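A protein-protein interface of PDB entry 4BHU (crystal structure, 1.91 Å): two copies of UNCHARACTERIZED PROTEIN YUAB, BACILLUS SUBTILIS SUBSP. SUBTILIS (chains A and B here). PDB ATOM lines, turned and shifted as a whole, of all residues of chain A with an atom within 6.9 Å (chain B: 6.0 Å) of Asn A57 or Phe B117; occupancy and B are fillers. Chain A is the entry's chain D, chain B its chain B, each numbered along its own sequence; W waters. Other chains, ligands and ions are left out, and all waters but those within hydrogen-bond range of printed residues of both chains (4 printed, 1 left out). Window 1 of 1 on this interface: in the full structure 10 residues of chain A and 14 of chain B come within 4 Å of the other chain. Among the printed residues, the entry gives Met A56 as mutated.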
ATOM      1  N   PHE A  42      15.890  13.261   9.137  1.00  0.00           N
ATOM      2  CA  PHE A  42      17.238  13.836   9.041  1.00  0.00           C
ATOM      3  C   PHE A  42      18.113  12.933   8.171  1.00  0.00           C
ATOM      4  O   PHE A  42      17.964  11.718   8.214  1.00  0.00           O
ATOM      5  CB  PHE A  42      17.899  13.868  10.412  1.00  0.00           C
ATOM      6  CG  PHE A  42      17.269  14.800  11.413  1.00  0.00           C
ATOM      7  CD1 PHE A  42      16.129  14.434  12.106  1.00  0.00           C
ATOM      8  CD2 PHE A  42      17.862  16.011  11.711  1.00  0.00           C
ATOM      9  CE1 PHE A  42      15.570  15.287  13.064  1.00  0.00           C
ATOM     10  CE2 PHE A  42      17.316  16.851  12.691  1.00  0.00           C
ATOM     11  CZ  PHE A  42      16.170  16.486  13.340  1.00  0.00           C
ATOM     12  N   THR A  55      20.341  10.624  20.472  1.00  0.00           N
ATOM     13  CA  THR A  55      19.026  10.930  21.031  1.00  0.00           C
ATOM     14  C   THR A  55      18.224  11.863  20.132  1.00  0.00           C
ATOM     15  O   THR A  55      18.777  12.640  19.346  1.00  0.00           O
ATOM     16  CB  THR A  55      19.116  11.576  22.432  1.00  0.00           C
ATOM     17  OG1 THR A  55      19.933  12.739  22.364  1.00  0.00           O
ATOM     18  CG2 THR A  55      19.693  10.608  23.478  1.00  0.00           C
ATOM     19  N   MET A  56      16.912  11.734  20.239  1.00  0.00           N
ATOM     20  CA  MET A  56      15.977  12.681  19.656  1.00  0.00           C
ATOM     21  C   MET A  56      15.153  13.264  20.799  1.00  0.00           C
ATOM     22  O   MET A  56      14.489  12.531  21.543  1.00  0.00           O
ATOM     23  CB  MET A  56      15.072  11.996  18.666  1.00  0.00           C
ATOM     24  CG  MET A  56      14.102  12.940  17.981  1.00  0.00           C
ATOM     25  SD  MET A  56      15.076  13.959  16.625  1.00  0.00           S
ATOM     26  CE  MET A  56      15.457  12.512  15.328  1.00  0.00           C
ATOM     27  N   ASN A  57      15.202  14.577  20.933  1.00  0.00           N
ATOM     28  CA  ASN A  57      14.525  15.293  22.027  1.00  0.00           C
ATOM     29  C   ASN A  57      14.803  14.627  23.378  1.00  0.00           C
ATOM     30  O   ASN A  57      13.893  14.422  24.188  1.00  0.00           O
ATOM     31  CB  ASN A  57      13.011  15.445  21.756  1.00  0.00           C
ATOM     32  CG  ASN A  57      12.732  16.368  20.570  1.00  0.00           C
ATOM     33  OD1 ASN A  57      13.443  16.314  19.568  1.00  0.00           O
ATOM     34  ND2 ASN A  57      11.740  17.251  20.696  1.00  0.00           N
ATOM     35  N   GLY A  58      16.069  14.248  23.574  1.00  0.00           N
ATOM     36  CA  GLY A  58      16.563  13.797  24.872  1.00  0.00           C
ATOM     37  C   GLY A  58      16.408  12.296  25.087  1.00  0.00           C
ATOM     38  O   GLY A  58      16.843  11.778  26.099  1.00  0.00           O
ATOM     39  N   ASN A  59      15.787  11.596  24.143  1.00  0.00           N
ATOM     40  CA  ASN A  59      15.484  10.172  24.316  1.00  0.00           C
ATOM     41  C   ASN A  59      16.241   9.336  23.294  1.00  0.00           C
ATOM     42  O   ASN A  59      16.322   9.714  22.127  1.00  0.00           O
ATOM     43  CB  ASN A  59      13.959   9.935  24.202  1.00  0.00           C
ATOM     44  CG  ASN A  59      13.515   8.552  24.718  1.00  0.00           C
ATOM     45  OD1 ASN A  59      14.176   7.931  25.545  1.00  0.00           O
ATOM     46  ND2 ASN A  59      12.381   8.096  24.239  1.00  0.00           N
ATOM     47  N   ALA A  60      16.786   8.199  23.733  1.00  0.00           N
ATOM     48  CA  ALA A  60      17.545   7.301  22.838  1.00  0.00           C
ATOM     49  C   ALA A  60      16.781   6.957  21.579  1.00  0.00           C
ATOM     50  O   ALA A  60      15.604   6.627  21.637  1.00  0.00           O
ATOM     51  CB  ALA A  60      17.904   6.004  23.568  1.00  0.00           C
ATOM     52  N   LEU A  61      17.467   7.008  20.440  1.00  0.00           N
ATOM     53  CA  LEU A  61      16.903   6.513  19.195  1.00  0.00           C
ATOM     54  C   LEU A  61      16.614   5.008  19.283  1.00  0.00           C
ATOM     55  O   LEU A  61      17.391   4.242  19.880  1.00  0.00           O
ATOM     56  CB  LEU A  61      17.851   6.780  18.021  1.00  0.00           C
ATOM     57  CG  LEU A  61      18.210   8.230  17.676  1.00  0.00           C
ATOM     58  CD1 LEU A  61      19.192   8.198  16.549  1.00  0.00           C
ATOM     59  CD2 LEU A  61      16.942   9.026  17.283  1.00  0.00           C
ATOM     60  N   VAL A  75      11.551  10.445  12.280  1.00  0.00           N
ATOM     61  CA  VAL A  75      10.510  10.618  13.279  1.00  0.00           C
ATOM     62  C   VAL A  75       9.198  10.298  12.549  1.00  0.00           C
ATOM     63  O   VAL A  75       8.678  11.125  11.813  1.00  0.00           O
ATOM     64  CB  VAL A  75      10.496  12.069  13.845  1.00  0.00           C
ATOM     65  CG1 VAL A  75       9.418  12.209  14.906  1.00  0.00           C
ATOM     66  CG2 VAL A  75      11.882  12.447  14.420  1.00  0.00           C
ATOM     67  N   GLU A  86       9.673  21.269  17.195  1.00  0.00           N
ATOM     68  CA  GLU A  86      11.122  21.249  17.134  1.00  0.00           C
ATOM     69  C   GLU A  86      11.659  19.838  17.444  1.00  0.00           C
ATOM     70  O   GLU A  86      11.232  19.179  18.398  1.00  0.00           O
ATOM     71  CB  GLU A  86      11.697  22.268  18.105  1.00  0.00           C
ATOM     72  CG  GLU A  86      13.203  22.364  18.126  1.00  0.00           C
ATOM     73  CD  GLU A  86      13.688  23.419  19.098  1.00  0.00           C
ATOM     74  OE1 GLU A  86      13.868  23.106  20.293  1.00  0.00           O
ATOM     75  OE2 GLU A  86      13.893  24.573  18.676  1.00  0.00           O
ATOM     76  N   PHE A  87      12.641  19.428  16.648  1.00  0.00           N
ATOM     77  CA  PHE A  87      13.285  18.130  16.752  1.00  0.00           C
ATOM     78  C   PHE A  87      14.776  18.350  16.887  1.00  0.00           C
ATOM     79  O   PHE A  87      15.377  19.027  16.067  1.00  0.00           O
ATOM     80  CB  PHE A  87      12.918  17.272  15.543  1.00  0.00           C
ATOM     81  CG  PHE A  87      11.444  17.225  15.316  1.00  0.00           C
ATOM     82  CD1 PHE A  87      10.654  16.348  16.019  1.00  0.00           C
ATOM     83  CD2 PHE A  87      10.843  18.153  14.511  1.00  0.00           C
ATOM     84  CE1 PHE A  87       9.273  16.357  15.848  1.00  0.00           C
ATOM     85  CE2 PHE A  87       9.480  18.181  14.368  1.00  0.00           C
ATOM     86  CZ  PHE A  87       8.701  17.270  15.042  1.00  0.00           C
ATOM     87  N   MLY A  88      15.342  17.849  17.988  1.00  0.00           N
ATOM     88  CA  MLY A  88      16.758  17.977  18.272  1.00  0.00           C
ATOM     89  CB  MLY A  88      16.969  18.625  19.624  1.00  0.00           C
ATOM     90  CG  MLY A  88      16.698  20.102  19.629  1.00  0.00           C
ATOM     91  CD  MLY A  88      17.207  20.755  20.887  1.00  0.00           C
ATOM     92  CE  MLY A  88      17.297  22.258  20.684  1.00  0.00           C
ATOM     93  NZ  MLY A  88      17.591  23.033  21.927  1.00  0.00           N
ATOM     94  CH1 MLY A  88      17.218  24.418  21.603  1.00  0.00           C
ATOM     95  CH2 MLY A  88      19.053  23.055  22.073  1.00  0.00           C
ATOM     96  C   MLY A  88      17.416  16.606  18.286  1.00  0.00           C
ATOM     97  O   MLY A  88      17.187  15.786  19.203  1.00  0.00           O
ATOM     98  N   LEU A  89      18.196  16.346  17.245  1.00  0.00           N
ATOM     99  CA  LEU A  89      18.941  15.106  17.150  1.00  0.00           C
ATOM    100  C   LEU A  89      20.334  15.377  17.679  1.00  0.00           C
ATOM    101  O   LEU A  89      21.020  16.304  17.218  1.00  0.00           O
ATOM    102  CB  LEU A  89      19.000  14.629  15.713  1.00  0.00           C
ATOM    103  CG  LEU A  89      19.933  13.452  15.424  1.00  0.00           C
ATOM    104  CD1 LEU A  89      19.561  12.218  16.176  1.00  0.00           C
ATOM    105  CD2 LEU A  89      19.924  13.154  13.938  1.00  0.00           C
ATOM    106  N   LYS A  90      20.733  14.610  18.684  1.00  0.00           N
ATOM    107  CA  LYS A  90      22.059  14.773  19.260  1.00  0.00           C
ATOM    108  C   LYS A  90      22.880  13.516  19.002  1.00  0.00           C
ATOM    109  O   LYS A  90      22.447  12.391  19.341  1.00  0.00           O
ATOM    110  CB  LYS A  90      21.989  15.039  20.747  1.00  0.00           C
ATOM    111  CG  LYS A  90      23.340  15.368  21.348  1.00  0.00           C
ATOM    112  CD  LYS A  90      23.245  15.853  22.799  1.00  0.00           C
ATOM    113  CE  LYS A  90      24.629  16.262  23.310  1.00  0.00           C
ATOM    114  NZ  LYS A  90      24.696  16.656  24.759  1.00  0.00           N
ATOM    115  N   ALA B   6       8.231  16.645  30.198  1.00  0.00           N
ATOM    116  CA  ALA B   6       7.245  15.733  30.748  1.00  0.00           C
ATOM    117  C   ALA B   6       7.663  15.430  32.166  1.00  0.00           C
ATOM    118  O   ALA B   6       8.855  15.425  32.490  1.00  0.00           O
ATOM    119  CB  ALA B   6       7.210  14.432  29.925  1.00  0.00           C
ATOM    120  N   TYR B  29       1.401  11.186  35.404  1.00  0.00           N
ATOM    121  CA  TYR B  29       2.153  11.659  34.262  1.00  0.00           C
ATOM    122  C   TYR B  29       1.565  12.928  33.653  1.00  0.00           C
ATOM    123  O   TYR B  29       0.371  13.010  33.375  1.00  0.00           O
ATOM    124  CB  TYR B  29       2.220  10.555  33.205  1.00  0.00           C
ATOM    125  CG  TYR B  29       2.940  10.939  31.934  1.00  0.00           C
ATOM    126  CD1 TYR B  29       4.315  11.154  31.917  1.00  0.00           C
ATOM    127  CD2 TYR B  29       2.250  11.056  30.751  1.00  0.00           C
ATOM    128  CE1 TYR B  29       4.982  11.486  30.732  1.00  0.00           C
ATOM    129  CE2 TYR B  29       2.905  11.390  29.579  1.00  0.00           C
ATOM    130  CZ  TYR B  29       4.263  11.599  29.584  1.00  0.00           C
ATOM    131  OH  TYR B  29       4.891  11.938  28.428  1.00  0.00           O
ATOM    132  N   PRO B  31       2.406  15.128  30.384  1.00  0.00           N
ATOM    133  CA  PRO B  31       3.194  15.217  29.144  1.00  0.00           C
ATOM    134  C   PRO B  31       3.845  16.572  28.965  1.00  0.00           C
ATOM    135  O   PRO B  31       4.926  16.653  28.363  1.00  0.00           O
ATOM    136  CB  PRO B  31       2.163  14.987  28.038  1.00  0.00           C
ATOM    137  CG  PRO B  31       0.969  14.440  28.697  1.00  0.00           C
ATOM    138  CD  PRO B  31       1.000  14.784  30.137  1.00  0.00           C
ATOM    139  N   THR B  33       3.066  19.143  26.989  1.00  0.00           N
ATOM    140  CA  THR B  33       3.217  19.368  25.563  1.00  0.00           C
ATOM    141  C   THR B  33       2.288  20.483  25.109  1.00  0.00           C
ATOM    142  O   THR B  33       1.184  20.659  25.634  1.00  0.00           O
ATOM    143  CB  THR B  33       2.957  18.074  24.732  1.00  0.00           C
ATOM    144  OG1 THR B  33       1.602  17.607  24.891  1.00  0.00           O
ATOM    145  CG2 THR B  33       3.936  16.967  25.107  1.00  0.00           C
ATOM    146  N   ALA B 106       6.976   6.756  31.813  1.00  0.00           N
ATOM    147  CA  ALA B 106       5.849   7.142  31.003  1.00  0.00           C
ATOM    148  C   ALA B 106       6.354   8.043  29.881  1.00  0.00           C
ATOM    149  O   ALA B 106       7.313   8.788  30.065  1.00  0.00           O
ATOM    150  CB  ALA B 106       4.796   7.841  31.829  1.00  0.00           C
ATOM    151  N   GLU B 107       5.707   7.966  28.726  1.00  0.00           N
ATOM    152  CA  GLU B 107       6.237   8.608  27.523  1.00  0.00           C
ATOM    153  C   GLU B 107       5.118   8.828  26.516  1.00  0.00           C
ATOM    154  O   GLU B 107       4.280   7.959  26.338  1.00  0.00           O
ATOM    155  CB  GLU B 107       7.296   7.715  26.852  1.00  0.00           C
ATOM    156  CG  GLU B 107       7.955   8.335  25.625  1.00  0.00           C
ATOM    157  CD  GLU B 107       8.964   7.409  24.933  1.00  0.00           C
ATOM    158  OE1 GLU B 107       9.352   6.392  25.533  1.00  0.00           O
ATOM    159  OE2 GLU B 107       9.354   7.706  23.778  1.00  0.00           O
ATOM    160  N   ASN B 108       5.151   9.977  25.852  1.00  0.00           N
ATOM    161  CA  ASN B 108       4.358  10.223  24.641  1.00  0.00           C
ATOM    162  C   ASN B 108       5.161   9.752  23.450  1.00  0.00           C
ATOM    163  O   ASN B 108       6.262  10.245  23.204  1.00  0.00           O
ATOM    164  CB  ASN B 108       4.037  11.704  24.477  1.00  0.00           C
ATOM    165  CG  ASN B 108       2.855  12.139  25.339  1.00  0.00           C
ATOM    166  OD1 ASN B 108       2.766  11.758  26.492  1.00  0.00           O
ATOM    167  ND2 ASN B 108       1.933  12.899  24.771  1.00  0.00           N
ATOM    168  N   LYS B 109       4.629   8.768  22.740  1.00  0.00           N
ATOM    169  CA  LYS B 109       5.397   8.054  21.717  1.00  0.00           C
ATOM    170  C   LYS B 109       5.137   8.534  20.298  1.00  0.00           C
ATOM    171  O   LYS B 109       5.848   8.153  19.364  1.00  0.00           O
ATOM    172  CB  LYS B 109       5.117   6.551  21.829  1.00  0.00           C
ATOM    173  CG  LYS B 109       5.816   5.939  23.045  1.00  0.00           C
ATOM    174  CD  LYS B 109       5.936   4.444  22.909  1.00  0.00           C
ATOM    175  CE  LYS B 109       6.763   3.844  24.045  1.00  0.00           C
ATOM    176  NZ  LYS B 109       6.830   2.335  23.931  1.00  0.00           N
ATOM    177  N   SER B 112       3.132  14.451  19.217  1.00  0.00           N
ATOM    178  CA  SER B 112       3.255  15.406  20.316  1.00  0.00           C
ATOM    179  C   SER B 112       4.269  16.472  20.030  1.00  0.00           C
ATOM    180  O   SER B 112       5.320  16.201  19.436  1.00  0.00           O
ATOM    181  CB  SER B 112       3.694  14.720  21.608  1.00  0.00           C
ATOM    182  OG  SER B 112       2.830  13.683  21.931  1.00  0.00           O
ATOM    183  N   ILE B 113       3.961  17.696  20.438  1.00  0.00           N
ATOM    184  CA  ILE B 113       4.913  18.795  20.328  1.00  0.00           C
ATOM    185  C   ILE B 113       5.509  19.041  21.718  1.00  0.00           C
ATOM    186  O   ILE B 113       4.788  19.279  22.669  1.00  0.00           O
ATOM    187  CB  ILE B 113       4.240  20.083  19.848  1.00  0.00           C
ATOM    188  CG1 ILE B 113       3.680  19.899  18.418  1.00  0.00           C
ATOM    189  CG2 ILE B 113       5.205  21.298  19.930  1.00  0.00           C
ATOM    190  CD1 ILE B 113       2.833  21.067  17.978  1.00  0.00           C
ATOM    191  N   GLY B 114       6.823  18.970  21.817  1.00  0.00           N
ATOM    192  CA  GLY B 114       7.485  19.139  23.100  1.00  0.00           C
ATOM    193  C   GLY B 114       8.988  18.974  23.032  1.00  0.00           C
ATOM    194  O   GLY B 114       9.541  18.614  21.985  1.00  0.00           O
ATOM    195  N   ASN B 115       9.651  19.242  24.161  1.00  0.00           N
ATOM    196  CA  ASN B 115      11.116  19.225  24.216  1.00  0.00           C
ATOM    197  C   ASN B 115      11.688  17.934  24.754  1.00  0.00           C
ATOM    198  O   ASN B 115      12.832  17.562  24.443  1.00  0.00           O
ATOM    199  CB  ASN B 115      11.613  20.380  25.029  1.00  0.00           C
ATOM    200  CG  ASN B 115      11.111  21.726  24.506  1.00  0.00           C
ATOM    201  OD1 ASN B 115      10.968  21.955  23.282  1.00  0.00           O
ATOM    202  ND2 ASN B 115      10.862  22.626  25.435  1.00  0.00           N
ATOM    203  N   MLY B 116      10.881  17.240  25.557  1.00  0.00           N
ATOM    204  CA  MLY B 116      11.276  15.978  26.154  1.00  0.00           C
ATOM    205  CB  MLY B 116      12.085  16.199  27.443  1.00  0.00           C
ATOM    206  CG  MLY B 116      12.634  14.929  28.031  1.00  0.00           C
ATOM    207  CD  MLY B 116      13.466  15.191  29.298  1.00  0.00           C
ATOM    208  CE  MLY B 116      13.926  13.905  29.909  1.00  0.00           C
ATOM    209  NZ  MLY B 116      14.613  14.126  31.250  1.00  0.00           N
ATOM    210  CH1 MLY B 116      15.870  14.825  30.962  1.00  0.00           C
ATOM    211  CH2 MLY B 116      14.997  12.792  31.749  1.00  0.00           C
ATOM    212  C   MLY B 116       9.977  15.233  26.455  1.00  0.00           C
ATOM    213  O   MLY B 116       9.145  15.752  27.176  1.00  0.00           O
ATOM    214  N   PHE B 117       9.827  14.039  25.893  1.00  0.00           N
ATOM    215  CA  PHE B 117       8.551  13.328  25.890  1.00  0.00           C
ATOM    216  C   PHE B 117       8.463  12.118  26.809  1.00  0.00           C
ATOM    217  O   PHE B 117       7.519  11.308  26.671  1.00  0.00           O
ATOM    218  CB  PHE B 117       8.247  12.798  24.494  1.00  0.00           C
ATOM    219  CG  PHE B 117       8.187  13.855  23.426  1.00  0.00           C
ATOM    220  CD1 PHE B 117       7.174  14.788  23.415  1.00  0.00           C
ATOM    221  CD2 PHE B 117       9.125  13.890  22.426  1.00  0.00           C
ATOM    222  CE1 PHE B 117       7.097  15.741  22.430  1.00  0.00           C
ATOM    223  CE2 PHE B 117       9.059  14.841  21.437  1.00  0.00           C
ATOM    224  CZ  PHE B 117       8.031  15.766  21.440  1.00  0.00           C
ATOM    225  N   TYR B 118       9.439  11.950  27.689  1.00  0.00           N
ATOM    226  CA  TYR B 118       9.407  10.821  28.603  1.00  0.00           C
ATOM    227  C   TYR B 118       9.836  11.295  29.966  1.00  0.00           C
ATOM    228  O   TYR B 118      10.446  12.356  30.112  1.00  0.00           O
ATOM    229  CB  TYR B 118      10.296   9.672  28.122  1.00  0.00           C
ATOM    230  CG  TYR B 118      11.764   9.894  28.359  1.00  0.00           C
ATOM    231  CD1 TYR B 118      12.506  10.675  27.500  1.00  0.00           C
ATOM    232  CD2 TYR B 118      12.406   9.322  29.440  1.00  0.00           C
ATOM    233  CE1 TYR B 118      13.828  10.889  27.704  1.00  0.00           C
ATOM    234  CE2 TYR B 118      13.732   9.543  29.672  1.00  0.00           C
ATOM    235  CZ  TYR B 118      14.445  10.330  28.789  1.00  0.00           C
ATOM    236  OH  TYR B 118      15.776  10.569  28.975  1.00  0.00           O
ATOM    237  N   ALA B 119       9.473  10.505  30.964  1.00  0.00           N
ATOM    238  CA  ALA B 119       9.785  10.823  32.346  1.00  0.00           C
ATOM    239  C   ALA B 119       9.849   9.512  33.112  1.00  0.00           C
ATOM    240  O   ALA B 119       9.187   8.524  32.743  1.00  0.00           O
ATOM    241  CB  ALA B 119       8.742  11.726  32.939  1.00  0.00           C
HETATM  242  O   HOH W   1       8.394  19.176  19.153  1.00  0.00           O
HETATM  243  O   HOH W   2      11.947  12.676  24.567  1.00  0.00           O
HETATM  244  O   HOH W   3      15.427  17.063  25.687  1.00  0.00           O
HETATM  245  O   HOH W   4      13.105  20.990  21.604  1.00  0.00           O
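The backbone carbonyl oxygen (O) of Gly A58 lies within hydrogen-bond range of the side-chain hydroxyl (OH) of Tyr B118, at 3.3 Å.
O of Gly B114 is in hydrogen-bond range of ND2 of Asn A57 (2.9 Å).
The side-chain carboxylate (OE2) of Glu B107 is in hydrogen-bond range of the side-chain amide nitrogen (ND2) of Asn A59, 3.1 Å away.
The backbone carbonyl oxygen of Asn A57 sits close to the backbone carbonyl oxygen of Asn B115.
The backbone NH of Asn A57 sits at hydrogen-bond distance from O of MLY A88.
The backbone NH of Asn B108 sits at hydrogen-bond distance from the backbone carbonyl oxygen of Phe B117.
O of MLY B116 is in hydrogen-bond range of N of Ala B6 (3.3 Å).
O of Phe B117 sits at hydrogen-bond distance from OH of Tyr B29 (3.2 Å).
The side-chain amide nitrogen of Asn A57 lies within hydrogen-bond range of the backbone carbonyl oxygen of Glu A86 (3.0 Å).
Among the printed residues, merely in contact across the chains: Asn A57 with MLY B116, Asn A59 with Tyr B118 and Asn A57 with Phe B117.
Asn A57 touches four residues of chain B.
Phe B117 touches just one residue of chain A: Asn A57 (3.7 Å).
Printed residues of chain B within 4 Å of Asn A59: Glu B107 (3.1 Å) and Tyr B118 (3.6 Å).
Of the printed residues of chain A, Tyr B118 touches Gly A58 (3.3 Å) and Asn A59 (3.6 Å).
Of the printed residues of chain A, Glu B107 touches Asn A59 (3.1 Å).
Of the printed residues of chain A, MLY B116 touches Asn A57.
Asn B108 touches none of the printed residues of chain A.
Glu A86 touches none of the printed residues of chain B.
The nearest printed residue of chain A that does not touch Tyr B118 is Asn A57 (5.0 Å).
Of the 14 printed residues of chain A, 3 touch a printed residue of chain B.
Of the 16 printed residues of chain B, 6 touch a printed residue of chain A.
Hydrophobic or aromatic side chains of chain B within 4 Å of the printed part of chain A: Phe B117 and Tyr B118.
Among the printed residues, 7 pairs touch across the chains.
Among the printed residues, no Asp or Glu carboxylate lies within 4 Å of a Lys or Arg side-chain nitrogen of the other chain.
No position is printed for both chains.
Water W4 bridges OE1 of Glu A86 (2.6 Å) and OD1 of Asn B115 (2.9 Å).
Water W2 bridges O of Asn A57 (2.6 Å) and N of Phe B117 (2.8 Å).
Water W3 lies within hydrogen-bond range of O of Asn B115 and O of Asn A57.
Water W1 bridges O of Glu A86 and N of Gly B114.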
